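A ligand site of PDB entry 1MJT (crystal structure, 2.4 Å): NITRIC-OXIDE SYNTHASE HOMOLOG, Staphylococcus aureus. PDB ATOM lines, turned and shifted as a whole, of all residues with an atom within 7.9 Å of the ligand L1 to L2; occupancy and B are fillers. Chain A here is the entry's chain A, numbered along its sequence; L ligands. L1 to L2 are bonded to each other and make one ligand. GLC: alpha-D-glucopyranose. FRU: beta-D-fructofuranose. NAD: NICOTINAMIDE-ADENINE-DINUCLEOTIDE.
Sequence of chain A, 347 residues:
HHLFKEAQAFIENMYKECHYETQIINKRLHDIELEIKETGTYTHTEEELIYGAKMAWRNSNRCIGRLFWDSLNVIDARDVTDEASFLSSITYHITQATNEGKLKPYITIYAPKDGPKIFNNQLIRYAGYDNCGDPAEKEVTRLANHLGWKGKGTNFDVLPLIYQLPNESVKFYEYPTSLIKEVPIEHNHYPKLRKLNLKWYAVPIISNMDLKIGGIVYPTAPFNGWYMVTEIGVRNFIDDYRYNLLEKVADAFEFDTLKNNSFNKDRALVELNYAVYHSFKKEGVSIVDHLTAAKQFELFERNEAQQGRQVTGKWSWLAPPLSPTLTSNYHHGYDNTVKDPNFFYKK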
ATOM      1  N   PHE A 297     -35.168 -16.652   6.264  1.00  0.00           N
ATOM      2  CA  PHE A 297     -34.274 -17.639   5.695  1.00  0.00           C
ATOM      3  C   PHE A 297     -33.069 -17.857   6.613  1.00  0.00           C
ATOM      4  O   PHE A 297     -32.578 -18.977   6.732  1.00  0.00           O
ATOM      5  CB  PHE A 297     -33.794 -17.214   4.315  1.00  0.00           C
ATOM      6  CG  PHE A 297     -33.073 -18.306   3.576  1.00  0.00           C
ATOM      7  CD1 PHE A 297     -33.738 -19.502   3.240  1.00  0.00           C
ATOM      8  CD2 PHE A 297     -31.735 -18.166   3.211  1.00  0.00           C
ATOM      9  CE1 PHE A 297     -33.068 -20.541   2.563  1.00  0.00           C
ATOM     10  CE2 PHE A 297     -31.057 -19.202   2.541  1.00  0.00           C
ATOM     11  CZ  PHE A 297     -31.738 -20.385   2.216  1.00  0.00           C
ATOM     12  N   GLU A 301     -31.626 -21.312   8.310  1.00  0.00           N
ATOM     13  CA  GLU A 301     -30.225 -21.708   8.328  1.00  0.00           C
ATOM     14  C   GLU A 301     -29.772 -22.000   9.741  1.00  0.00           C
ATOM     15  O   GLU A 301     -28.987 -22.916   9.975  1.00  0.00           O
ATOM     16  CB  GLU A 301     -29.360 -20.625   7.680  1.00  0.00           C
ATOM     17  CG  GLU A 301     -29.632 -20.479   6.206  1.00  0.00           C
ATOM     18  CD  GLU A 301     -28.658 -19.557   5.503  1.00  0.00           C
ATOM     19  OE1 GLU A 301     -28.877 -18.326   5.494  1.00  0.00           O
ATOM     20  OE2 GLU A 301     -27.653 -20.090   4.973  1.00  0.00           O
ATOM     21  N   GLU A 304     -31.362 -25.285  10.911  1.00  0.00           N
ATOM     22  CA  GLU A 304     -30.768 -26.449  10.253  1.00  0.00           C
ATOM     23  C   GLU A 304     -29.434 -26.830  10.890  1.00  0.00           C
ATOM     24  O   GLU A 304     -29.170 -28.014  11.130  1.00  0.00           O
ATOM     25  CB  GLU A 304     -30.555 -26.177   8.756  1.00  0.00           C
ATOM     26  CG  GLU A 304     -31.811 -26.205   7.901  1.00  0.00           C
ATOM     27  CD  GLU A 304     -32.477 -27.584   7.847  1.00  0.00           C
ATOM     28  OE1 GLU A 304     -33.329 -27.874   8.709  1.00  0.00           O
ATOM     29  OE2 GLU A 304     -32.132 -28.369   6.931  1.00  0.00           O
ATOM     30  N   ALA A 305     -28.596 -25.838  11.151  1.00  0.00           N
ATOM     31  CA  ALA A 305     -27.292 -26.059  11.764  1.00  0.00           C
ATOM     32  C   ALA A 305     -27.449 -26.680  13.147  1.00  0.00           C
ATOM     33  O   ALA A 305     -26.601 -27.465  13.581  1.00  0.00           O
ATOM     34  CB  ALA A 305     -26.540 -24.748  11.871  1.00  0.00           C
ATOM     35  N   ARG A 309     -27.666 -30.288  10.221  1.00  0.00           N
ATOM     36  CA  ARG A 309     -27.739 -30.316   8.767  1.00  0.00           C
ATOM     37  C   ARG A 309     -27.132 -29.065   8.147  1.00  0.00           C
ATOM     38  O   ARG A 309     -27.254 -27.962   8.699  1.00  0.00           O
ATOM     39  CB  ARG A 309     -29.195 -30.448   8.311  1.00  0.00           C
ATOM     40  CG  ARG A 309     -29.810 -31.819   8.584  1.00  0.00           C
ATOM     41  CD  ARG A 309     -31.108 -31.990   7.820  1.00  0.00           C
ATOM     42  NE  ARG A 309     -32.178 -31.156   8.342  1.00  0.00           N
ATOM     43  CZ  ARG A 309     -32.743 -31.324   9.530  1.00  0.00           C
ATOM     44  NH1 ARG A 309     -32.322 -32.302  10.316  1.00  0.00           N
ATOM     45  NH2 ARG A 309     -33.738 -30.530   9.931  1.00  0.00           N
ATOM     46  N   GLN A 310     -26.465 -29.233   7.015  1.00  0.00           N
ATOM     47  CA  GLN A 310     -25.868 -28.102   6.329  1.00  0.00           C
ATOM     48  C   GLN A 310     -26.912 -27.557   5.357  1.00  0.00           C
ATOM     49  O   GLN A 310     -27.884 -28.241   5.039  1.00  0.00           O
ATOM     50  CB  GLN A 310     -24.606 -28.510   5.570  1.00  0.00           C
ATOM     51  CG  GLN A 310     -24.857 -29.451   4.418  1.00  0.00           C
ATOM     52  CD  GLN A 310     -24.068 -29.074   3.180  1.00  0.00           C
ATOM     53  OE1 GLN A 310     -24.089 -29.794   2.174  1.00  0.00           O
ATOM     54  NE2 GLN A 310     -23.377 -27.935   3.233  1.00  0.00           N
ATOM     55  N   VAL A 311     -26.700 -26.326   4.882  1.00  0.00           N
ATOM     56  CA  VAL A 311     -27.642 -25.716   3.973  1.00  0.00           C
ATOM     57  C   VAL A 311     -27.133 -25.556   2.552  1.00  0.00           C
ATOM     58  O   VAL A 311     -26.077 -24.977   2.293  1.00  0.00           O
ATOM     59  CB  VAL A 311     -28.098 -24.322   4.471  1.00  0.00           C
ATOM     60  CG1 VAL A 311     -29.036 -23.678   3.459  1.00  0.00           C
ATOM     61  CG2 VAL A 311     -28.807 -24.470   5.813  1.00  0.00           C
ATOM     62  N   THR A 312     -27.930 -26.084   1.622  1.00  0.00           N
ATOM     63  CA  THR A 312     -27.628 -26.002   0.218  1.00  0.00           C
ATOM     64  C   THR A 312     -28.565 -24.954  -0.391  1.00  0.00           C
ATOM     65  O   THR A 312     -29.632 -24.679   0.172  1.00  0.00           O
ATOM     66  CB  THR A 312     -27.878 -27.346  -0.461  1.00  0.00           C
ATOM     67  OG1 THR A 312     -29.210 -27.768  -0.166  1.00  0.00           O
ATOM     68  CG2 THR A 312     -26.887 -28.392   0.050  1.00  0.00           C
ATOM     69  N   GLY A 313     -28.168 -24.382  -1.518  1.00  0.00           N
ATOM     70  CA  GLY A 313     -29.003 -23.375  -2.172  1.00  0.00           C
ATOM     71  C   GLY A 313     -28.401 -22.815  -3.444  1.00  0.00           C
ATOM     72  O   GLY A 313     -27.194 -22.934  -3.661  1.00  0.00           O
ATOM     73  N   LYS A 314     -29.231 -22.216  -4.287  1.00  0.00           N
ATOM     74  CA  LYS A 314     -28.743 -21.621  -5.513  1.00  0.00           C
ATOM     75  C   LYS A 314     -28.752 -20.103  -5.365  1.00  0.00           C
ATOM     76  O   LYS A 314     -29.794 -19.466  -5.463  1.00  0.00           O
ATOM     77  CB  LYS A 314     -29.599 -22.035  -6.715  1.00  0.00           C
ATOM     78  CG  LYS A 314     -28.954 -21.706  -8.039  1.00  0.00           C
ATOM     79  CD  LYS A 314     -29.770 -22.195  -9.212  1.00  0.00           C
ATOM     80  CE  LYS A 314     -29.068 -21.896 -10.524  1.00  0.00           C
ATOM     81  NZ  LYS A 314     -27.723 -22.536 -10.586  1.00  0.00           N
ATOM     82  N   LEU A 318     -32.026 -17.349  -4.553  1.00  0.00           N
ATOM     83  CA  LEU A 318     -32.272 -16.863  -3.195  1.00  0.00           C
ATOM     84  C   LEU A 318     -32.157 -15.339  -3.087  1.00  0.00           C
ATOM     85  O   LEU A 318     -32.822 -14.722  -2.242  1.00  0.00           O
ATOM     86  CB  LEU A 318     -31.277 -17.511  -2.239  1.00  0.00           C
ATOM     87  CG  LEU A 318     -31.371 -19.037  -2.163  1.00  0.00           C
ATOM     88  CD1 LEU A 318     -30.218 -19.597  -1.340  1.00  0.00           C
ATOM     89  CD2 LEU A 318     -32.713 -19.430  -1.576  1.00  0.00           C
ATOM     90  N   SER A 328     -28.912 -11.034   3.766  1.00  0.00           N
ATOM     91  CA  SER A 328     -27.697 -11.725   4.191  1.00  0.00           C
ATOM     92  C   SER A 328     -27.123 -12.673   3.142  1.00  0.00           C
ATOM     93  O   SER A 328     -25.929 -12.651   2.875  1.00  0.00           O
ATOM     94  CB  SER A 328     -27.968 -12.513   5.468  1.00  0.00           C
ATOM     95  OG  SER A 328     -26.817 -13.220   5.861  1.00  0.00           O
ATOM     96  N   ASN A 329     -27.997 -13.493   2.551  1.00  0.00           N
ATOM     97  CA  ASN A 329     -27.586 -14.479   1.549  1.00  0.00           C
ATOM     98  C   ASN A 329     -26.887 -13.889   0.330  1.00  0.00           C
ATOM     99  O   ASN A 329     -26.188 -14.593  -0.388  1.00  0.00           O
ATOM    100  CB  ASN A 329     -28.791 -15.305   1.091  1.00  0.00           C
ATOM    101  CG  ASN A 329     -29.941 -14.468   0.623  1.00  0.00           C
ATOM    102  OD1 ASN A 329     -30.689 -13.922   1.430  1.00  0.00           O
ATOM    103  ND2 ASN A 329     -30.097 -14.351  -0.680  1.00  0.00           N
ATOM    104  N   HIS A 332     -22.586 -14.061   0.450  1.00  0.00           N
ATOM    105  CA  HIS A 332     -21.751 -15.256   0.481  1.00  0.00           C
ATOM    106  C   HIS A 332     -22.334 -16.288  -0.465  1.00  0.00           C
ATOM    107  O   HIS A 332     -23.465 -16.144  -0.920  1.00  0.00           O
ATOM    108  CB  HIS A 332     -21.612 -15.830   1.899  1.00  0.00           C
ATOM    109  CG  HIS A 332     -22.892 -16.307   2.496  1.00  0.00           C
ATOM    110  ND1 HIS A 332     -23.815 -15.460   3.055  1.00  0.00           N
ATOM    111  CD2 HIS A 332     -23.391 -17.555   2.638  1.00  0.00           C
ATOM    112  CE1 HIS A 332     -24.833 -16.163   3.522  1.00  0.00           C
ATOM    113  NE2 HIS A 332     -24.608 -17.444   3.278  1.00  0.00           N
ATOM    114  N   GLY A 333     -21.556 -17.317  -0.784  1.00  0.00           N
ATOM    115  CA  GLY A 333     -22.029 -18.330  -1.702  1.00  0.00           C
ATOM    116  C   GLY A 333     -22.755 -19.461  -1.018  1.00  0.00           C
ATOM    117  O   GLY A 333     -22.754 -19.576   0.208  1.00  0.00           O
ATOM    118  N   TYR A 334     -23.392 -20.295  -1.828  1.00  0.00           N
ATOM    119  CA  TYR A 334     -24.133 -21.453  -1.340  1.00  0.00           C
ATOM    120  C   TYR A 334     -23.707 -22.696  -2.108  1.00  0.00           C
ATOM    121  O   TYR A 334     -23.270 -22.617  -3.253  1.00  0.00           O
ATOM    122  CB  TYR A 334     -25.641 -21.236  -1.496  1.00  0.00           C
ATOM    123  CG  TYR A 334     -26.243 -20.354  -0.425  1.00  0.00           C
ATOM    124  CD1 TYR A 334     -26.738 -20.894   0.745  1.00  0.00           C
ATOM    125  CD2 TYR A 334     -26.237 -18.965  -0.569  1.00  0.00           C
ATOM    126  CE1 TYR A 334     -27.211 -20.074   1.780  1.00  0.00           C
ATOM    127  CE2 TYR A 334     -26.700 -18.136   0.451  1.00  0.00           C
ATOM    128  CZ  TYR A 334     -27.190 -18.699   1.625  1.00  0.00           C
ATOM    129  OH  TYR A 334     -27.611 -17.872   2.648  1.00  0.00           O
ATOM    130  N   ASP A 335     -23.841 -23.841  -1.449  1.00  0.00           N
ATOM    131  CA  ASP A 335     -23.518 -25.112  -2.060  1.00  0.00           C
ATOM    132  C   ASP A 335     -24.766 -25.584  -2.800  1.00  0.00           C
ATOM    133  O   ASP A 335     -25.730 -26.020  -2.200  1.00  0.00           O
ATOM    134  CB  ASP A 335     -23.110 -26.110  -0.974  1.00  0.00           C
ATOM    135  CG  ASP A 335     -22.949 -27.508  -1.494  1.00  0.00           C
ATOM    136  OD1 ASP A 335     -22.328 -27.679  -2.564  1.00  0.00           O
ATOM    137  OD2 ASP A 335     -23.444 -28.443  -0.833  1.00  0.00           O
ATOM    138  N   ASN A 336     -24.735 -25.456  -4.120  1.00  0.00           N
ATOM    139  CA  ASN A 336     -25.867 -25.821  -4.972  1.00  0.00           C
ATOM    140  C   ASN A 336     -26.091 -27.324  -5.123  1.00  0.00           C
ATOM    141  O   ASN A 336     -26.803 -27.755  -6.026  1.00  0.00           O
ATOM    142  CB  ASN A 336     -25.670 -25.199  -6.366  1.00  0.00           C
ATOM    143  CG  ASN A 336     -26.955 -25.157  -7.186  1.00  0.00           C
ATOM    144  OD1 ASN A 336     -26.923 -24.847  -8.380  1.00  0.00           O
ATOM    145  ND2 ASN A 336     -28.081 -25.456  -6.557  1.00  0.00           N
ATOM    146  N   THR A 337     -25.485 -28.118  -4.250  1.00  0.00           N
ATOM    147  CA  THR A 337     -25.647 -29.569  -4.322  1.00  0.00           C
ATOM    148  C   THR A 337     -27.109 -29.948  -4.130  1.00  0.00           C
ATOM    149  O   THR A 337     -27.751 -29.578  -3.137  1.00  0.00           O
ATOM    150  CB  THR A 337     -24.807 -30.312  -3.250  1.00  0.00           C
ATOM    151  OG1 THR A 337     -23.419 -30.250  -3.609  1.00  0.00           O
ATOM    152  CG2 THR A 337     -25.239 -31.760  -3.136  1.00  0.00           C
HETATM  153  C1  GLC L   1     -20.968 -22.061   5.371  1.00  0.00           C
HETATM  154  C2  GLC L   1     -19.773 -22.639   6.158  1.00  0.00           C
HETATM  155  C3  GLC L   1     -19.780 -24.198   6.113  1.00  0.00           C
HETATM  156  C4  GLC L   1     -21.081 -24.744   6.653  1.00  0.00           C
HETATM  157  C5  GLC L   1     -22.289 -24.124   5.908  1.00  0.00           C
HETATM  158  C6  GLC L   1     -23.586 -24.522   6.526  1.00  0.00           C
HETATM  159  O2  GLC L   1     -18.570 -22.092   5.586  1.00  0.00           O
HETATM  160  O3  GLC L   1     -18.695 -24.661   6.900  1.00  0.00           O
HETATM  161  O4  GLC L   1     -21.066 -26.199   6.491  1.00  0.00           O
HETATM  162  O5  GLC L   1     -22.200 -22.658   5.946  1.00  0.00           O
HETATM  163  O6  GLC L   1     -24.563 -24.763   5.519  1.00  0.00           O
HETATM  164  C1  FRU L   2     -20.409 -20.567   2.343  1.00  0.00           C
HETATM  165  C2  FRU L   2     -21.415 -21.570   2.902  1.00  0.00           C
HETATM  166  C3  FRU L   2     -22.012 -22.566   1.855  1.00  0.00           C
HETATM  167  C4  FRU L   2     -23.397 -22.833   2.386  1.00  0.00           C
HETATM  168  C5  FRU L   2     -23.781 -21.424   2.893  1.00  0.00           C
HETATM  169  C6  FRU L   2     -24.845 -21.341   3.974  1.00  0.00           C
HETATM  170  O1  FRU L   2     -19.362 -21.287   1.704  1.00  0.00           O
HETATM  171  O2  FRU L   2     -20.815 -22.404   3.970  1.00  0.00           O
HETATM  172  O3  FRU L   2     -21.233 -23.727   1.624  1.00  0.00           O
HETATM  173  O4  FRU L   2     -24.236 -23.289   1.327  1.00  0.00           O
HETATM  174  O5  FRU L   2     -22.533 -20.857   3.382  1.00  0.00           O
HETATM  175  O6  FRU L   2     -25.062 -20.034   4.450  1.00  0.00           O
HETATM  176  PA  NAD L   3     -19.184 -18.918  -6.716  1.00  0.00           P
HETATM  177  O1A NAD L   3     -18.633 -17.635  -6.191  1.00  0.00           O
HETATM  178  O2A NAD L   3     -19.080 -20.138  -5.848  1.00  0.00           O
HETATM  179  O5B NAD L   3     -18.463 -19.172  -8.196  1.00  0.00           O
HETATM  180  O3  NAD L   3     -20.759 -18.798  -7.138  1.00  0.00           O
HETATM  181  PN  NAD L   3     -21.797 -17.612  -7.501  1.00  0.00           P
HETATM  182  O1N NAD L   3     -21.362 -16.887  -8.718  1.00  0.00           O
HETATM  183  O2N NAD L   3     -23.118 -18.407  -7.441  1.00  0.00           O
HETATM  184  O5D NAD L   3     -21.564 -16.676  -6.198  1.00  0.00           O
HETATM  185  C5D NAD L   3     -22.048 -15.379  -6.091  1.00  0.00           C
HETATM  186  C4D NAD L   3     -21.082 -14.660  -5.208  1.00  0.00           C
HETATM  187  O4D NAD L   3     -20.654 -13.454  -5.909  1.00  0.00           O
HETATM  188  C3D NAD L   3     -21.689 -14.192  -3.859  1.00  0.00           C
HETATM  189  O3D NAD L   3     -21.021 -14.915  -2.824  1.00  0.00           O
HETATM  190  C2D NAD L   3     -21.482 -12.661  -3.831  1.00  0.00           C
HETATM  191  O2D NAD L   3     -21.137 -12.100  -2.542  1.00  0.00           O
HETATM  192  C1D NAD L   3     -20.430 -12.408  -4.897  1.00  0.00           C
HETATM  193  N1N NAD L   3     -20.543 -11.136  -5.643  1.00  0.00           N
HETATM  194  C2N NAD L   3     -19.491 -10.241  -5.302  1.00  0.00           C
HETATM  195  C3N NAD L   3     -19.508  -8.947  -5.903  1.00  0.00           C
HETATM  196  C7N NAD L   3     -18.452  -7.836  -5.597  1.00  0.00           C
HETATM  197  O7N NAD L   3     -17.780  -7.893  -4.545  1.00  0.00           O
HETATM  198  N7N NAD L   3     -18.279  -6.821  -6.487  1.00  0.00           N
HETATM  199  C4N NAD L   3     -20.542  -8.527  -6.859  1.00  0.00           C
HETATM  200  C5N NAD L   3     -21.545  -9.525  -7.126  1.00  0.00           C
HETATM  201  C6N NAD L   3     -21.626 -10.803  -6.577  1.00  0.00           C
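An oxygen (O4) of FRU L2 lies within hydrogen-bond range of the backbone carbonyl oxygen (O) of Val 311, 2.7 Å away.
The backbone NH of Gly 333 sits at hydrogen-bond distance from an oxygen (O3D) of NAD L3, at 3.2 Å.
N of Val 311 sits at hydrogen-bond distance from O6 of GLC L1 (2.7 Å).
An oxygen (O4) of FRU L2 is in hydrogen-bond range of the backbone NH of Asp 335.
The side-chain carboxylate (OE2) of Glu 301 is in hydrogen-bond range of an oxygen (O6) of FRU L2, 2.6 Å away.
A ring nitrogen (NE2) of His 332 sits at hydrogen-bond distance from an oxygen (O6) of FRU L2 (2.9 Å).
The backbone carbonyl oxygen (O) of His 332 lies close to an oxygen (O3D) of NAD L3 (3.3 Å).
OD1 of Asp 335 sits at hydrogen-bond distance from OG1 of Thr 337.
The backbone carbonyl oxygen of Asp 335 is in hydrogen-bond range of the backbone NH of Gly 313 (3.0 Å).
OD2 of Asp 335 lies close to OE1 of Gln 310 (3.4 Å).
A ring nitrogen (NE2) of His 332 sits at hydrogen-bond distance from the side-chain hydroxyl (OH) of Tyr 334 (3.1 Å).
The side-chain carboxylate (OE1) of Glu 301 sits at hydrogen-bond distance from the side-chain hydroxyl (OH) of Tyr 334, at 3.1 Å.
An oxygen (O5) of FRU L2 sits close to the backbone carbonyl oxygen (O) of Gly 333, at 3.4 Å.
Merely in contact with the ligand L1 to L2: Gln 310 and Tyr 334.
Seven residues have an atom within 4 Å of the ligand L1 to L2: Glu 301, Gln 310, Val 311, His 332, Gly 333, Tyr 334 and Asp 335.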
